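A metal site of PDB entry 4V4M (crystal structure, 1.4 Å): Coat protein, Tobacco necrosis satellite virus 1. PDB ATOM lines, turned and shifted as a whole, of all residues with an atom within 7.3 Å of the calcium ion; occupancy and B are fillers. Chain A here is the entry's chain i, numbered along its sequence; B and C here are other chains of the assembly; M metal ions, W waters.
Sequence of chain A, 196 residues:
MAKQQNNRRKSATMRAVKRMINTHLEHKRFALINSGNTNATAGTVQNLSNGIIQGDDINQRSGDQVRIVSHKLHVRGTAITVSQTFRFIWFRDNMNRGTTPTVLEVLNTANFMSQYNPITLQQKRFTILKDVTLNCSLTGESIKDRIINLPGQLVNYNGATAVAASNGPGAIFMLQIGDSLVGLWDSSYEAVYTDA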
ATOM      1  N   LYS A  28     -20.182  -1.722  -2.682  1.00  0.00           N
ATOM      2  CA  LYS A  28     -21.137  -2.692  -3.221  1.00  0.00           C
ATOM      3  C   LYS A  28     -22.522  -2.334  -2.720  1.00  0.00           C
ATOM      4  O   LYS A  28     -22.681  -1.537  -1.804  1.00  0.00           O
ATOM      5  CB  LYS A  28     -20.720  -4.107  -2.805  1.00  0.00           C
ATOM      6  CG  LYS A  28     -19.381  -4.520  -3.427  1.00  0.00           C
ATOM      7  CD  LYS A  28     -19.060  -5.985  -3.199  1.00  0.00           C
ATOM      8  CE  LYS A  28     -17.815  -6.382  -3.976  1.00  0.00           C
ATOM      9  NZ  LYS A  28     -17.256  -7.736  -3.581  1.00  0.00           N
ATOM     10  N   ARG A  61     -20.628 -10.985  -1.690  1.00  0.00           N
ATOM     11  CA  ARG A  61     -19.497 -10.700  -0.811  1.00  0.00           C
ATOM     12  C   ARG A  61     -18.385 -11.722  -0.970  1.00  0.00           C
ATOM     13  O   ARG A  61     -18.622 -12.878  -1.346  1.00  0.00           O
ATOM     14  CB  ARG A  61     -19.923 -10.642   0.669  1.00  0.00           C
ATOM     15  CG  ARG A  61     -20.516 -11.959   1.166  1.00  0.00           C
ATOM     16  CD  ARG A  61     -20.979 -11.899   2.601  1.00  0.00           C
ATOM     17  NE  ARG A  61     -22.028 -12.900   2.822  1.00  0.00           N
ATOM     18  CZ  ARG A  61     -21.835 -14.132   3.333  1.00  0.00           C
ATOM     19  NH1 ARG A  61     -20.620 -14.552   3.663  1.00  0.00           N
ATOM     20  NH2 ARG A  61     -22.871 -14.945   3.458  1.00  0.00           N
ATOM     21  N   SER A  62     -17.163 -11.271  -0.689  1.00  0.00           N
ATOM     22  CA  SER A  62     -15.998 -12.141  -0.532  1.00  0.00           C
ATOM     23  C   SER A  62     -15.814 -12.398   0.965  1.00  0.00           C
ATOM     24  O   SER A  62     -15.808 -11.462   1.762  1.00  0.00           O
ATOM     25  CB  SER A  62     -14.765 -11.413  -1.092  1.00  0.00           C
ATOM     26  OG  SER A  62     -13.666 -12.281  -1.082  1.00  0.00           O
ATOM     27  N   GLY A  63     -15.658 -13.657   1.358  1.00  0.00           N
ATOM     28  CA  GLY A  63     -15.460 -13.988   2.777  1.00  0.00           C
ATOM     29  C   GLY A  63     -16.721 -13.815   3.596  1.00  0.00           C
ATOM     30  O   GLY A  63     -17.828 -13.809   3.065  1.00  0.00           O
ATOM     31  N   ASP A  64     -16.540 -13.663   4.909  1.00  0.00           N
ATOM     32  CA  ASP A  64     -17.653 -13.704   5.846  1.00  0.00           C
ATOM     33  C   ASP A  64     -17.825 -12.373   6.597  1.00  0.00           C
ATOM     34  O   ASP A  64     -18.470 -12.322   7.657  1.00  0.00           O
ATOM     35  CB  ASP A  64     -17.485 -14.865   6.839  1.00  0.00           C
ATOM     36  CG  ASP A  64     -17.933 -16.194   6.256  1.00  0.00           C
ATOM     37  OD1 ASP A  64     -18.734 -16.205   5.294  1.00  0.00           O
ATOM     38  OD2 ASP A  64     -17.489 -17.250   6.785  1.00  0.00           O
ATOM     39  N   GLN A  65     -17.277 -11.297   6.039  1.00  0.00           N
ATOM     40  CA  GLN A  65     -17.491  -9.950   6.597  1.00  0.00           C
ATOM     41  C   GLN A  65     -17.793  -8.950   5.502  1.00  0.00           C
ATOM     42  O   GLN A  65     -17.227  -9.033   4.413  1.00  0.00           O
ATOM     43  CB  GLN A  65     -16.255  -9.444   7.389  1.00  0.00           C
ATOM     44  CG  GLN A  65     -16.047 -10.108   8.750  1.00  0.00           C
ATOM     45  CD  GLN A  65     -14.973  -9.406   9.571  1.00  0.00           C
ATOM     46  OE1 GLN A  65     -14.109  -8.716   9.033  1.00  0.00           O
ATOM     47  NE2 GLN A  65     -15.029  -9.557  10.884  1.00  0.00           N
ATOM     48  N   VAL A  66     -18.715  -8.029   5.778  1.00  0.00           N
ATOM     49  CA  VAL A  66     -18.790  -6.776   5.026  1.00  0.00           C
ATOM     50  C   VAL A  66     -18.980  -5.643   6.035  1.00  0.00           C
ATOM     51  O   VAL A  66     -19.260  -5.874   7.206  1.00  0.00           O
ATOM     52  CB  VAL A  66     -19.975  -6.748   4.023  1.00  0.00           C
ATOM     53  CG1 VAL A  66     -19.853  -7.884   2.974  1.00  0.00           C
ATOM     54  CG2 VAL A  66     -21.344  -6.750   4.748  1.00  0.00           C
ATOM     55  N   ARG A  67     -18.859  -4.409   5.565  1.00  0.00           N
ATOM     56  CA  ARG A  67     -19.077  -3.261   6.438  1.00  0.00           C
ATOM     57  C   ARG A  67     -20.127  -2.354   5.815  1.00  0.00           C
ATOM     58  O   ARG A  67     -19.893  -1.742   4.769  1.00  0.00           O
ATOM     59  CB  ARG A  67     -17.770  -2.486   6.619  1.00  0.00           C
ATOM     60  CG  ARG A  67     -16.718  -3.252   7.412  1.00  0.00           C
ATOM     61  CD  ARG A  67     -15.481  -2.389   7.575  1.00  0.00           C
ATOM     62  NE  ARG A  67     -15.848  -1.004   7.856  1.00  0.00           N
ATOM     63  CZ  ARG A  67     -15.022   0.025   7.759  1.00  0.00           C
ATOM     64  NH1 ARG A  67     -13.755  -0.181   7.393  1.00  0.00           N
ATOM     65  NH2 ARG A  67     -15.443   1.251   8.037  1.00  0.00           N
ATOM     66  N   VAL A 155     -20.798  -6.386   9.511  1.00  0.00           N
ATOM     67  CA  VAL A 155     -21.642  -7.576   9.535  1.00  0.00           C
ATOM     68  C   VAL A 155     -20.796  -8.825   9.345  1.00  0.00           C
ATOM     69  O   VAL A 155     -20.076  -8.912   8.358  1.00  0.00           O
ATOM     70  CB  VAL A 155     -22.686  -7.579   8.388  1.00  0.00           C
ATOM     71  CG1 VAL A 155     -23.616  -8.782   8.554  1.00  0.00           C
ATOM     72  CG2 VAL A 155     -23.507  -6.251   8.401  1.00  0.00           C
ATOM     73  N   THR A 194     -18.888  -1.788   2.031  1.00  0.00           N
ATOM     74  CA  THR A 194     -17.583  -2.180   1.515  1.00  0.00           C
ATOM     75  C   THR A 194     -17.271  -3.627   1.865  1.00  0.00           C
ATOM     76  O   THR A 194     -17.866  -4.218   2.792  1.00  0.00           O
ATOM     77  CB  THR A 194     -16.475  -1.275   2.001  1.00  0.00           C
ATOM     78  OG1 THR A 194     -16.352  -1.368   3.430  1.00  0.00           O
ATOM     79  CG2 THR A 194     -16.761   0.203   1.620  1.00  0.00           C
ATOM     80  N   ASP A 195     -16.328  -4.185   1.126  1.00  0.00           N
ATOM     81  CA  ASP A 195     -16.052  -5.608   1.185  1.00  0.00           C
ATOM     82  C   ASP A 195     -14.569  -5.852   0.935  1.00  0.00           C
ATOM     83  O   ASP A 195     -14.190  -6.730   0.146  1.00  0.00           O
ATOM     84  CB  ASP A 195     -16.883  -6.295   0.088  1.00  0.00           C
ATOM     85  CG  ASP A 195     -16.838  -7.808   0.181  1.00  0.00           C
ATOM     86  OD1 ASP A 195     -16.993  -8.464  -0.863  1.00  0.00           O
ATOM     87  OD2 ASP A 195     -16.664  -8.336   1.310  1.00  0.00           O
ATOM     88  N   ALA A 196     -13.729  -5.085   1.619  1.00  0.00           N
ATOM     89  CA  ALA A 196     -12.284  -5.079   1.390  1.00  0.00           C
ATOM     90  C   ALA A 196     -11.556  -6.079   2.276  1.00  0.00           C
ATOM     91  O   ALA A 196     -10.354  -6.242   2.123  1.00  0.00           O
ATOM     92  CB  ALA A 196     -11.730  -3.695   1.629  1.00  0.00           C
ATOM     93  OXT ALA A 196     -12.104  -6.707   3.188  1.00  0.00           O
ATOM     94  N   LEU B  25     -10.445  -3.821   6.549  1.00  0.00           N
ATOM     95  CA  LEU B  25     -10.116  -5.042   5.804  1.00  0.00           C
ATOM     96  C   LEU B  25     -10.525  -6.299   6.553  1.00  0.00           C
ATOM     97  O   LEU B  25     -10.225  -6.441   7.740  1.00  0.00           O
ATOM     98  CB  LEU B  25      -8.603  -5.125   5.542  1.00  0.00           C
ATOM     99  CG  LEU B  25      -7.927  -3.878   4.994  1.00  0.00           C
ATOM    100  CD1 LEU B  25      -6.449  -4.175   4.689  1.00  0.00           C
ATOM    101  CD2 LEU B  25      -8.645  -3.408   3.747  1.00  0.00           C
ATOM    102  N   GLU B  26     -11.171  -7.223   5.838  1.00  0.00           N
ATOM    103  CA  GLU B  26     -11.509  -8.502   6.462  1.00  0.00           C
ATOM    104  C   GLU B  26     -10.241  -9.310   6.745  1.00  0.00           C
ATOM    105  O   GLU B  26      -9.373  -9.473   5.881  1.00  0.00           O
ATOM    106  CB  GLU B  26     -12.470  -9.317   5.588  1.00  0.00           C
ATOM    107  CG  GLU B  26     -12.815 -10.698   6.187  1.00  0.00           C
ATOM    108  CD  GLU B  26     -13.873 -11.475   5.417  1.00  0.00           C
ATOM    109  OE1 GLU B  26     -14.601 -10.883   4.600  1.00  0.00           O
ATOM    110  OE2 GLU B  26     -13.959 -12.710   5.626  1.00  0.00           O
ATOM    111  N   LYS B  28      -9.353 -12.614   6.954  1.00  0.00           N
ATOM    112  CA  LYS B  28      -9.678 -13.972   6.632  1.00  0.00           C
ATOM    113  C   LYS B  28      -8.794 -14.909   7.463  1.00  0.00           C
ATOM    114  O   LYS B  28      -7.812 -14.470   8.069  1.00  0.00           O
ATOM    115  CB  LYS B  28      -9.514 -14.189   5.129  1.00  0.00           C
ATOM    116  CG  LYS B  28     -10.592 -13.454   4.318  1.00  0.00           C
ATOM    117  CD  LYS B  28     -10.462 -13.696   2.795  1.00  0.00           C
ATOM    118  CE  LYS B  28     -11.514 -12.885   2.014  1.00  0.00           C
ATOM    119  NZ  LYS B  28     -11.407 -13.061   0.553  1.00  0.00           N
ATOM    120  N   ASP B  56     -14.369 -17.707  -2.723  1.00  0.00           N
ATOM    121  CA  ASP B  56     -15.065 -16.647  -2.008  1.00  0.00           C
ATOM    122  C   ASP B  56     -15.221 -16.891  -0.496  1.00  0.00           C
ATOM    123  O   ASP B  56     -15.797 -16.061   0.219  1.00  0.00           O
ATOM    124  CB  ASP B  56     -16.460 -16.455  -2.618  1.00  0.00           C
ATOM    125  CG  ASP B  56     -16.401 -16.188  -4.120  1.00  0.00           C
ATOM    126  OD1 ASP B  56     -15.437 -15.535  -4.583  1.00  0.00           O
ATOM    127  OD2 ASP B  56     -17.322 -16.644  -4.824  1.00  0.00           O
ATOM    128  N   GLN C 122     -12.908 -15.192  13.889  1.00  0.00           N
ATOM    129  CA  GLN C 122     -12.963 -13.977  13.086  1.00  0.00           C
ATOM    130  C   GLN C 122     -13.954 -12.988  13.676  1.00  0.00           C
ATOM    131  O   GLN C 122     -13.673 -11.790  13.760  1.00  0.00           O
ATOM    132  CB  GLN C 122     -13.365 -14.266  11.626  1.00  0.00           C
ATOM    133  CG  GLN C 122     -13.524 -12.973  10.816  1.00  0.00           C
ATOM    134  CD  GLN C 122     -14.055 -13.199   9.410  1.00  0.00           C
ATOM    135  OE1 GLN C 122     -15.246 -13.488   9.231  1.00  0.00           O
ATOM    136  NE2 GLN C 122     -13.186 -13.060   8.424  1.00  0.00           N
HETATM  137 CA    CA M   1     -15.468  -9.521   2.899  1.00  0.00          CA
HETATM  138  O   HOH W   1     -14.630  -7.428   3.775  1.00  0.00           O
HETATM  139  O   HOH W   2     -13.498  -9.175   1.510  1.00  0.00           O
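The backbone NH (N) of Asp 64 sits at hydrogen-bond distance from the side-chain carboxylate (OE2) of Glu 26 of chain B (2.8 Å).
OE2 of Glu 26 of chain B lies within hydrogen-bond range of NE2 of Gln 122 of chain C, at 2.9 Å.
The side-chain carboxylate (OD1) of Asp 195 is in salt-bridge range of the side-chain amino group (NZ) of Lys 28 of chain A (2.8 Å).
OG of Ser 62 lies within hydrogen-bond range of NZ of Lys 28 of chain B, 2.9 Å away.
The backbone NH of Glu 26 of chain B is in hydrogen-bond range of the chain-end carboxylate of Ala 196, at 2.9 Å.
Within 4 Å of the calcium ion: Ser 62, Gln 65, Asp 195 and Glu 26 of chain B.
The nearest printed residue that does not touch the calcium ion is Ala 196 (4.4 Å).
The calcium ion is bound by the backbone carbonyl oxygen (O) of Ser 62, at 2.3 Å.
OD2 of Asp 195 binds the calcium ion.
The side-chain carboxylate (OE1) of Glu 26 of chain B is bound to the calcium ion (2.3 Å).
The calcium ion is bound by O of Gln 65 (2.4 Å).
The calcium ion is bound by water W1, at 2.4 Å.
Water W2 is bound to the calcium ion (2.4 Å).
The calcium ion has six donor atoms within binding distance.
Water W2 lies within hydrogen-bond range of the backbone carbonyl oxygen (O) of Asp 195 and the chain-end carboxylate (OXT) of Ala 196.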
